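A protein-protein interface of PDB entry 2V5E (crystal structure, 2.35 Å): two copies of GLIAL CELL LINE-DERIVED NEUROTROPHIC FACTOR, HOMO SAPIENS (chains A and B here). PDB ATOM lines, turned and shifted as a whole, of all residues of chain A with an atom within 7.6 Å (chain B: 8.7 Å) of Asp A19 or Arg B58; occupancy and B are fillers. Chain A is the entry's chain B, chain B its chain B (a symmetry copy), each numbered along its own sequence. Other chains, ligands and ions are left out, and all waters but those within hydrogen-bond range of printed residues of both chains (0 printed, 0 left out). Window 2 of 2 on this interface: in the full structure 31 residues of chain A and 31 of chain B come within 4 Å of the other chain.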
ATOM      1  N   ILE A  13      17.788  23.577   0.420  1.00  0.00           N
ATOM      2  CA  ILE A  13      16.718  23.219  -0.507  1.00  0.00           C
ATOM      3  C   ILE A  13      15.343  23.776  -0.128  1.00  0.00           C
ATOM      4  O   ILE A  13      14.971  23.853   1.055  1.00  0.00           O
ATOM      5  CB  ILE A  13      16.608  21.687  -0.762  1.00  0.00           C
ATOM      6  CG1 ILE A  13      16.542  20.923   0.561  1.00  0.00           C
ATOM      7  CG2 ILE A  13      17.771  21.207  -1.647  1.00  0.00           C
ATOM      8  CD1 ILE A  13      16.238  19.457   0.408  1.00  0.00           C
ATOM      9  N   HIS A  14      14.601  24.145  -1.162  1.00  0.00           N
ATOM     10  CA  HIS A  14      13.284  24.719  -1.025  1.00  0.00           C
ATOM     11  C   HIS A  14      12.239  23.580  -1.019  1.00  0.00           C
ATOM     12  O   HIS A  14      12.189  22.760  -1.937  1.00  0.00           O
ATOM     13  CB  HIS A  14      13.069  25.736  -2.167  1.00  0.00           C
ATOM     14  CG  HIS A  14      11.752  26.449  -2.118  1.00  0.00           C
ATOM     15  ND1 HIS A  14      11.185  27.034  -3.231  1.00  0.00           N
ATOM     16  CD2 HIS A  14      10.881  26.652  -1.099  1.00  0.00           C
ATOM     17  CE1 HIS A  14      10.026  27.573  -2.898  1.00  0.00           C
ATOM     18  NE2 HIS A  14       9.818  27.354  -1.609  1.00  0.00           N
ATOM     19  N   LEU A  15      11.419  23.538   0.026  1.00  0.00           N
ATOM     20  CA  LEU A  15      10.501  22.428   0.251  1.00  0.00           C
ATOM     21  C   LEU A  15       9.107  22.891   0.673  1.00  0.00           C
ATOM     22  O   LEU A  15       8.941  23.975   1.243  1.00  0.00           O
ATOM     23  CB  LEU A  15      11.048  21.520   1.353  1.00  0.00           C
ATOM     24  CG  LEU A  15      12.354  20.735   1.162  1.00  0.00           C
ATOM     25  CD1 LEU A  15      12.693  20.021   2.463  1.00  0.00           C
ATOM     26  CD2 LEU A  15      12.289  19.739  -0.005  1.00  0.00           C
ATOM     27  N   ASN A  16       8.108  22.062   0.394  1.00  0.00           N
ATOM     28  CA  ASN A  16       6.834  22.152   1.093  1.00  0.00           C
ATOM     29  C   ASN A  16       7.049  21.557   2.486  1.00  0.00           C
ATOM     30  O   ASN A  16       7.872  20.642   2.642  1.00  0.00           O
ATOM     31  CB  ASN A  16       5.744  21.377   0.339  1.00  0.00           C
ATOM     32  CG  ASN A  16       5.429  21.985  -1.022  1.00  0.00           C
ATOM     33  OD1 ASN A  16       5.006  23.128  -1.098  1.00  0.00           O
ATOM     34  ND2 ASN A  16       5.636  21.212  -2.099  1.00  0.00           N
ATOM     35  N   VAL A  17       6.337  22.061   3.496  1.00  0.00           N
ATOM     36  CA  VAL A  17       6.420  21.470   4.829  1.00  0.00           C
ATOM     37  C   VAL A  17       5.985  19.989   4.783  1.00  0.00           C
ATOM     38  O   VAL A  17       6.476  19.158   5.554  1.00  0.00           O
ATOM     39  CB  VAL A  17       5.603  22.277   5.877  1.00  0.00           C
ATOM     40  CG1 VAL A  17       5.463  21.520   7.194  1.00  0.00           C
ATOM     41  CG2 VAL A  17       6.252  23.644   6.133  1.00  0.00           C
ATOM     42  N   THR A  18       5.072  19.657   3.872  1.00  0.00           N
ATOM     43  CA  THR A  18       4.566  18.277   3.770  1.00  0.00           C
ATOM     44  C   THR A  18       5.637  17.277   3.317  1.00  0.00           C
ATOM     45  O   THR A  18       5.549  16.101   3.651  1.00  0.00           O
ATOM     46  CB  THR A  18       3.342  18.164   2.847  1.00  0.00           C
ATOM     47  OG1 THR A  18       3.582  18.904   1.644  1.00  0.00           O
ATOM     48  CG2 THR A  18       2.121  18.694   3.533  1.00  0.00           C
ATOM     49  N   ASP A  19       6.650  17.760   2.591  1.00  0.00           N
ATOM     50  CA  ASP A  19       7.770  16.934   2.109  1.00  0.00           C
ATOM     51  C   ASP A  19       8.627  16.362   3.225  1.00  0.00           C
ATOM     52  O   ASP A  19       9.369  15.402   3.012  1.00  0.00           O
ATOM     53  CB  ASP A  19       8.660  17.754   1.165  1.00  0.00           C
ATOM     54  CG  ASP A  19       7.905  18.244  -0.071  1.00  0.00           C
ATOM     55  OD1 ASP A  19       6.954  17.555  -0.490  1.00  0.00           O
ATOM     56  OD2 ASP A  19       8.243  19.319  -0.611  1.00  0.00           O
ATOM     57  N   LEU A  20       8.520  16.951   4.412  1.00  0.00           N
ATOM     58  CA  LEU A  20       9.353  16.565   5.551  1.00  0.00           C
ATOM     59  C   LEU A  20       8.906  15.271   6.191  1.00  0.00           C
ATOM     60  O   LEU A  20       9.649  14.678   6.966  1.00  0.00           O
ATOM     61  CB  LEU A  20       9.326  17.663   6.618  1.00  0.00           C
ATOM     62  CG  LEU A  20       9.762  19.075   6.220  1.00  0.00           C
ATOM     63  CD1 LEU A  20       9.630  19.961   7.457  1.00  0.00           C
ATOM     64  CD2 LEU A  20      11.187  19.104   5.675  1.00  0.00           C
ATOM     65  N   GLY A  21       7.681  14.858   5.885  1.00  0.00           N
ATOM     66  CA  GLY A  21       7.082  13.666   6.472  1.00  0.00           C
ATOM     67  C   GLY A  21       6.933  13.676   7.983  1.00  0.00           C
ATOM     68  O   GLY A  21       7.023  12.620   8.603  1.00  0.00           O
ATOM     69  N   LEU A  22       6.711  14.852   8.581  1.00  0.00           N
ATOM     70  CA  LEU A  22       6.648  14.968  10.044  1.00  0.00           C
ATOM     71  C   LEU A  22       5.232  14.910  10.626  1.00  0.00           C
ATOM     72  O   LEU A  22       5.055  15.114  11.844  1.00  0.00           O
ATOM     73  CB  LEU A  22       7.382  16.236  10.543  1.00  0.00           C
ATOM     74  CG  LEU A  22       8.882  16.372  10.233  1.00  0.00           C
ATOM     75  CD1 LEU A  22       9.498  17.553  10.944  1.00  0.00           C
ATOM     76  CD2 LEU A  22       9.667  15.065  10.553  1.00  0.00           C
ATOM     77  N   TYR A  24       2.418  16.692   9.294  1.00  0.00           N
ATOM     78  CA  TYR A  24       1.688  17.945   9.138  1.00  0.00           C
ATOM     79  C   TYR A  24       0.874  17.962   7.872  1.00  0.00           C
ATOM     80  O   TYR A  24       1.296  17.397   6.859  1.00  0.00           O
ATOM     81  CB  TYR A  24       2.644  19.148   9.096  1.00  0.00           C
ATOM     82  CG  TYR A  24       3.486  19.317  10.336  1.00  0.00           C
ATOM     83  CD1 TYR A  24       2.896  19.562  11.574  1.00  0.00           C
ATOM     84  CD2 TYR A  24       4.882  19.245  10.266  1.00  0.00           C
ATOM     85  CE1 TYR A  24       3.668  19.721  12.709  1.00  0.00           C
ATOM     86  CE2 TYR A  24       5.666  19.403  11.408  1.00  0.00           C
ATOM     87  CZ  TYR A  24       5.050  19.640  12.621  1.00  0.00           C
ATOM     88  OH  TYR A  24       5.819  19.792  13.749  1.00  0.00           O
ATOM     89  N   THR A  26      -0.553  20.885   5.554  1.00  0.00           N
ATOM     90  CA  THR A  26      -0.442  22.321   5.363  1.00  0.00           C
ATOM     91  C   THR A  26       0.099  22.619   3.978  1.00  0.00           C
ATOM     92  O   THR A  26       0.787  21.774   3.389  1.00  0.00           O
ATOM     93  CB  THR A  26       0.501  22.952   6.417  1.00  0.00           C
ATOM     94  OG1 THR A  26       0.616  24.361   6.182  1.00  0.00           O
ATOM     95  CG2 THR A  26       1.877  22.306   6.365  1.00  0.00           C
ATOM     96  N   GLU A  28       2.002  25.288   3.528  1.00  0.00           N
ATOM     97  CA  GLU A  28       3.151  26.176   3.787  1.00  0.00           C
ATOM     98  C   GLU A  28       4.500  25.563   3.374  1.00  0.00           C
ATOM     99  O   GLU A  28       4.594  24.355   3.129  1.00  0.00           O
ATOM    100  CB  GLU A  28       3.149  26.666   5.242  1.00  0.00           C
ATOM    101  CG  GLU A  28       1.956  27.586   5.565  1.00  0.00           C
ATOM    102  CD  GLU A  28       2.330  28.770   6.443  1.00  0.00           C
ATOM    103  OE1 GLU A  28       3.456  29.287   6.304  1.00  0.00           O
ATOM    104  OE2 GLU A  28       1.494  29.187   7.277  1.00  0.00           O
ATOM    105  N   LEU A  30       9.203  26.022   3.256  1.00  0.00           N
ATOM    106  CA  LEU A  30      10.424  26.370   4.001  1.00  0.00           C
ATOM    107  C   LEU A  30      11.668  26.220   3.128  1.00  0.00           C
ATOM    108  O   LEU A  30      11.602  25.648   2.033  1.00  0.00           O
ATOM    109  CB  LEU A  30      10.579  25.499   5.263  1.00  0.00           C
ATOM    110  CG  LEU A  30      11.005  24.016   5.145  1.00  0.00           C
ATOM    111  CD1 LEU A  30      11.655  23.501   6.423  1.00  0.00           C
ATOM    112  CD2 LEU A  30       9.846  23.116   4.732  1.00  0.00           C
ATOM    113  N   TYR A  34      21.040  21.347   5.134  1.00  0.00           N
ATOM    114  CA  TYR A  34      21.666  20.180   5.731  1.00  0.00           C
ATOM    115  C   TYR A  34      23.176  20.199   5.526  1.00  0.00           C
ATOM    116  O   TYR A  34      23.688  20.884   4.647  1.00  0.00           O
ATOM    117  CB  TYR A  34      21.041  18.868   5.180  1.00  0.00           C
ATOM    118  CG  TYR A  34      21.244  18.675   3.695  1.00  0.00           C
ATOM    119  CD1 TYR A  34      20.346  19.213   2.773  1.00  0.00           C
ATOM    120  CD2 TYR A  34      22.361  17.984   3.212  1.00  0.00           C
ATOM    121  CE1 TYR A  34      20.543  19.044   1.398  1.00  0.00           C
ATOM    122  CE2 TYR A  34      22.579  17.821   1.853  1.00  0.00           C
ATOM    123  CZ  TYR A  34      21.665  18.352   0.956  1.00  0.00           C
ATOM    124  OH  TYR A  34      21.880  18.191  -0.377  1.00  0.00           O
ATOM    125  N   LYS B  48      15.189  12.806  11.159  1.00  0.00           N
ATOM    126  CA  LYS B  48      13.934  12.308  10.573  1.00  0.00           C
ATOM    127  C   LYS B  48      13.717  12.948   9.205  1.00  0.00           C
ATOM    128  O   LYS B  48      13.406  12.249   8.233  1.00  0.00           O
ATOM    129  CB  LYS B  48      12.729  12.537  11.493  1.00  0.00           C
ATOM    130  CG  LYS B  48      12.743  11.693  12.765  1.00  0.00           C
ATOM    131  CD  LYS B  48      11.552  12.008  13.673  1.00  0.00           C
ATOM    132  CE  LYS B  48      11.566  11.162  14.948  1.00  0.00           C
ATOM    133  NZ  LYS B  48      10.376  11.463  15.827  1.00  0.00           N
ATOM    134  N   ILE B  49      13.922  14.265   9.119  1.00  0.00           N
ATOM    135  CA  ILE B  49      13.793  14.958   7.840  1.00  0.00           C
ATOM    136  C   ILE B  49      14.709  14.359   6.750  1.00  0.00           C
ATOM    137  O   ILE B  49      14.248  14.066   5.652  1.00  0.00           O
ATOM    138  CB  ILE B  49      14.007  16.478   7.970  1.00  0.00           C
ATOM    139  CG1 ILE B  49      12.930  17.098   8.866  1.00  0.00           C
ATOM    140  CG2 ILE B  49      13.973  17.145   6.602  1.00  0.00           C
ATOM    141  CD1 ILE B  49      13.259  18.528   9.321  1.00  0.00           C
ATOM    142  N   LEU B  50      15.986  14.161   7.065  1.00  0.00           N
ATOM    143  CA  LEU B  50      16.939  13.585   6.110  1.00  0.00           C
ATOM    144  C   LEU B  50      16.499  12.203   5.589  1.00  0.00           C
ATOM    145  O   LEU B  50      16.534  11.937   4.398  1.00  0.00           O
ATOM    146  CB  LEU B  50      18.340  13.498   6.723  1.00  0.00           C
ATOM    147  CG  LEU B  50      19.175  14.788   6.813  1.00  0.00           C
ATOM    148  CD1 LEU B  50      20.472  14.511   7.583  1.00  0.00           C
ATOM    149  CD2 LEU B  50      19.496  15.386   5.439  1.00  0.00           C
ATOM    150  N   LYS B  51      16.060  11.358   6.503  1.00  0.00           N
ATOM    151  CA  LYS B  51      15.622  10.013   6.211  1.00  0.00           C
ATOM    152  C   LYS B  51      14.358  10.034   5.344  1.00  0.00           C
ATOM    153  O   LYS B  51      14.237   9.269   4.370  1.00  0.00           O
ATOM    154  CB  LYS B  51      15.360   9.333   7.542  1.00  0.00           C
ATOM    155  CG  LYS B  51      15.237   7.870   7.506  1.00  0.00           C
ATOM    156  CD  LYS B  51      14.828   7.386   8.889  1.00  0.00           C
ATOM    157  CE  LYS B  51      14.921   5.864   9.001  1.00  0.00           C
ATOM    158  NZ  LYS B  51      14.194   5.132   7.910  1.00  0.00           N
ATOM    159  N   ASN B  52      13.436  10.932   5.683  1.00  0.00           N
ATOM    160  CA  ASN B  52      12.178  11.076   4.939  1.00  0.00           C
ATOM    161  C   ASN B  52      12.368  11.644   3.549  1.00  0.00           C
ATOM    162  O   ASN B  52      11.667  11.254   2.614  1.00  0.00           O
ATOM    163  CB  ASN B  52      11.166  11.906   5.726  1.00  0.00           C
ATOM    164  CG  ASN B  52      10.773  11.238   7.015  1.00  0.00           C
ATOM    165  OD1 ASN B  52      11.101  10.061   7.233  1.00  0.00           O
ATOM    166  ND2 ASN B  52      10.080  11.968   7.885  1.00  0.00           N
ATOM    167  N   LEU B  53      13.323  12.553   3.409  1.00  0.00           N
ATOM    168  CA  LEU B  53      13.617  13.123   2.102  1.00  0.00           C
ATOM    169  C   LEU B  53      14.321  12.123   1.164  1.00  0.00           C
ATOM    170  O   LEU B  53      14.172  12.232  -0.056  1.00  0.00           O
ATOM    171  CB  LEU B  53      14.428  14.415   2.229  1.00  0.00           C
ATOM    172  CG  LEU B  53      13.786  15.660   2.835  1.00  0.00           C
ATOM    173  CD1 LEU B  53      14.827  16.803   2.951  1.00  0.00           C
ATOM    174  CD2 LEU B  53      12.544  16.136   2.047  1.00  0.00           C
ATOM    175  N   SER B  54      15.086  11.171   1.714  1.00  0.00           N
ATOM    176  CA  SER B  54      15.643  10.090   0.888  1.00  0.00           C
ATOM    177  C   SER B  54      14.501   9.153   0.494  1.00  0.00           C
ATOM    178  O   SER B  54      14.389   8.753  -0.662  1.00  0.00           O
ATOM    179  CB  SER B  54      16.733   9.277   1.601  1.00  0.00           C
ATOM    180  OG  SER B  54      17.711  10.104   2.210  1.00  0.00           O
ATOM    181  N   ARG B  55      13.654   8.813   1.459  1.00  0.00           N
ATOM    182  CA  ARG B  55      12.526   7.935   1.185  1.00  0.00           C
ATOM    183  C   ARG B  55      11.613   8.463   0.077  1.00  0.00           C
ATOM    184  O   ARG B  55      11.251   7.693  -0.819  1.00  0.00           O
ATOM    185  CB  ARG B  55      11.730   7.626   2.447  1.00  0.00           C
ATOM    186  CG  ARG B  55      10.570   6.678   2.197  1.00  0.00           C
ATOM    187  CD  ARG B  55       9.894   6.300   3.500  1.00  0.00           C
ATOM    188  NE  ARG B  55       8.668   5.544   3.278  1.00  0.00           N
ATOM    189  CZ  ARG B  55       7.484   6.108   3.073  1.00  0.00           C
ATOM    190  NH1 ARG B  55       7.376   7.439   3.062  1.00  0.00           N
ATOM    191  NH2 ARG B  55       6.419   5.339   2.872  1.00  0.00           N
ATOM    192  N   ASN B  56      11.256   9.758   0.125  1.00  0.00           N
ATOM    193  CA  ASN B  56      10.339  10.344  -0.889  1.00  0.00           C
ATOM    194  C   ASN B  56      11.039  10.946  -2.114  1.00  0.00           C
ATOM    195  O   ASN B  56      10.410  11.600  -2.956  1.00  0.00           O
ATOM    196  CB  ASN B  56       9.262  11.286  -0.269  1.00  0.00           C
ATOM    197  CG  ASN B  56       9.835  12.598   0.322  1.00  0.00           C
ATOM    198  OD1 ASN B  56      10.888  13.103  -0.102  1.00  0.00           O
ATOM    199  ND2 ASN B  56       9.109  13.169   1.287  1.00  0.00           N
ATOM    200  N   ARG B  57      12.354  10.727  -2.176  1.00  0.00           N
ATOM    201  CA  ARG B  57      13.209  11.065  -3.326  1.00  0.00           C
ATOM    202  C   ARG B  57      13.462  12.561  -3.572  1.00  0.00           C
ATOM    203  O   ARG B  57      14.013  12.948  -4.602  1.00  0.00           O
ATOM    204  CB  ARG B  57      12.727  10.347  -4.601  1.00  0.00           C
ATOM    205  CG  ARG B  57      12.698   8.825  -4.465  1.00  0.00           C
ATOM    206  CD  ARG B  57      12.738   8.168  -5.833  1.00  0.00           C
ATOM    207  NE  ARG B  57      13.314   6.822  -5.802  1.00  0.00           N
ATOM    208  CZ  ARG B  57      14.606   6.548  -5.605  1.00  0.00           C
ATOM    209  NH1 ARG B  57      15.014   5.285  -5.609  1.00  0.00           N
ATOM    210  NH2 ARG B  57      15.491   7.524  -5.396  1.00  0.00           N
ATOM    211  N   ARG B  58      13.099  13.399  -2.608  1.00  0.00           N
ATOM    212  CA  ARG B  58      13.462  14.816  -2.666  1.00  0.00           C
ATOM    213  C   ARG B  58      14.974  15.015  -2.448  1.00  0.00           C
ATOM    214  O   ARG B  58      15.526  16.062  -2.785  1.00  0.00           O
ATOM    215  CB  ARG B  58      12.627  15.633  -1.680  1.00  0.00           C
ATOM    216  CG  ARG B  58      11.313  16.175  -2.270  1.00  0.00           C
ATOM    217  CD  ARG B  58      10.326  15.070  -2.591  1.00  0.00           C
ATOM    218  NE  ARG B  58       9.042  15.577  -3.070  1.00  0.00           N
ATOM    219  CZ  ARG B  58       8.016  14.808  -3.435  1.00  0.00           C
ATOM    220  NH1 ARG B  58       8.108  13.481  -3.371  1.00  0.00           N
ATOM    221  NH2 ARG B  58       6.892  15.363  -3.858  1.00  0.00           N
ATOM    222  N   LEU B  59      15.635  13.996  -1.898  1.00  0.00           N
ATOM    223  CA  LEU B  59      17.095  13.941  -1.867  1.00  0.00           C
ATOM    224  C   LEU B  59      17.593  12.809  -2.761  1.00  0.00           C
ATOM    225  O   LEU B  59      17.598  11.651  -2.349  1.00  0.00           O
ATOM    226  CB  LEU B  59      17.613  13.766  -0.433  1.00  0.00           C
ATOM    227  CG  LEU B  59      17.618  14.991   0.487  1.00  0.00           C
ATOM    228  CD1 LEU B  59      18.244  14.623   1.828  1.00  0.00           C
ATOM    229  CD2 LEU B  59      18.347  16.173  -0.144  1.00  0.00           C
ATOM    230  N   VAL B  60      17.994  13.147  -3.989  1.00  0.00           N
ATOM    231  CA  VAL B  60      18.434  12.153  -4.990  1.00  0.00           C
ATOM    232  C   VAL B  60      19.728  11.486  -4.505  1.00  0.00           C
ATOM    233  O   VAL B  60      20.826  11.809  -4.982  1.00  0.00           O
ATOM    234  CB  VAL B  60      18.629  12.784  -6.427  1.00  0.00           C
ATOM    235  CG1 VAL B  60      18.627  11.702  -7.512  1.00  0.00           C
ATOM    236  CG2 VAL B  60      17.559  13.841  -6.739  1.00  0.00           C
ATOM    237  N   SER B  61      19.577  10.574  -3.540  1.00  0.00           N
ATOM    238  CA  SER B  61      20.687   9.897  -2.845  1.00  0.00           C
ATOM    239  C   SER B  61      20.184   9.207  -1.573  1.00  0.00           C
ATOM    240  O   SER B  61      19.082   9.484  -1.103  1.00  0.00           O
ATOM    241  CB  SER B  61      21.804  10.884  -2.474  1.00  0.00           C
ATOM    242  OG  SER B  61      22.819  10.237  -1.722  1.00  0.00           O
ATOM    243  N   VAL B  64      22.865  10.426   2.980  1.00  0.00           N
ATOM    244  CA  VAL B  64      23.565  11.717   2.938  1.00  0.00           C
ATOM    245  C   VAL B  64      23.357  12.489   4.254  1.00  0.00           C
ATOM    246  O   VAL B  64      22.225  12.572   4.754  1.00  0.00           O
ATOM    247  CB  VAL B  64      23.133  12.569   1.692  1.00  0.00           C
ATOM    248  CG1 VAL B  64      21.739  13.181   1.884  1.00  0.00           C
ATOM    249  CG2 VAL B  64      24.171  13.644   1.372  1.00  0.00           C
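CD1 of Ile A13 touches CD1 of Leu B53, 3.9 Å away. Ile A13 touches Leu B59. Leu B53 touches Leu A15. CD2 of Leu B53 touches O of Asp A19, 3.4 Å away. CG2 of Ile B49 touches CD2 of Leu A20, at 3.5 Å. Tyr A34 touches Leu B50. Leu B59 touches Tyr A34.
Of the 15 printed residues of chain B, 7 touch a printed residue of chain A. Printed residues of chain A that touch a printed residue of chain B: Ile A13, Leu A15, Asp A19, Leu A20, Gly A21 and Tyr A34. Hydrophobic or aromatic side chains of chain A within 4 Å of the printed part of chain B: Ile A13, Leu A15, Leu A20 and Tyr A34. Among the printed residues, 11 pairs touch across the chains. Among the printed residues, Asp or Glu carboxylates within 4 Å of a Lys or Arg side-chain nitrogen of the other chain: Asp A19 with Arg B58 (3.9 Å).
OD2 of Asp A19 lies within hydrogen-bond range of N of Asn A16 (2.9 Å). The backbone carbonyl oxygen of Leu B50 is in hydrogen-bond range of the side-chain hydroxyl of Ser B54 (3.1 Å). The side-chain amide oxygen (OD1) of Asn B56 lies close to the backbone carbonyl oxygen (O) of Asn B52. The backbone carbonyl oxygen (O) of Leu B53 lies close to the side-chain amide oxygen (OD1) of Asn B56 (3.4 Å). N of Leu B59 is in hydrogen-bond range of O of Leu B53 (2.9 Å). O of Asn B56 is in hydrogen-bond range of NH1 of Arg B58 (3.0 Å).
Asp A19 touches just these residues of chain B: Leu B53, Asn B56 and Arg B58. Of the printed residues of chain A, Leu B50 touches Tyr A34. Printed residues of chain B within 4 Å of Tyr A34: Leu B50 (3.8 Å) and Leu B59 (3.9 Å). Of the printed residues of chain A, Leu B59 touches Ile A13 and Tyr A34. Of the printed residues of chain A, Asn B56 touches Asp A19. Of the printed residues of chain B, Gly A21 touches Asn B52 (3.2 Å). The nearest residue of chain B that does not touch Asp A19 is Asn B52 (4.8 Å). The nearest printed residue of chain A that does not touch Leu B50 is Leu A20 (6.4 Å).
No position is printed for both chains.
The backbone carbonyl oxygen (O) of Asp A19 lies within hydrogen-bond range of the side-chain amide nitrogen (ND2) of Asn B56. OD1 of Asp A19 lies within salt-bridge range of NE of Arg B58 (3.9 Å). The backbone carbonyl oxygen (O) of Leu A20 sits at hydrogen-bond distance from the side-chain amide nitrogen (ND2) of Asn B52. The backbone carbonyl oxygen (O) of Gly A21 is in hydrogen-bond range of the side-chain amide nitrogen (ND2) of Asn B52, at 3.2 Å.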
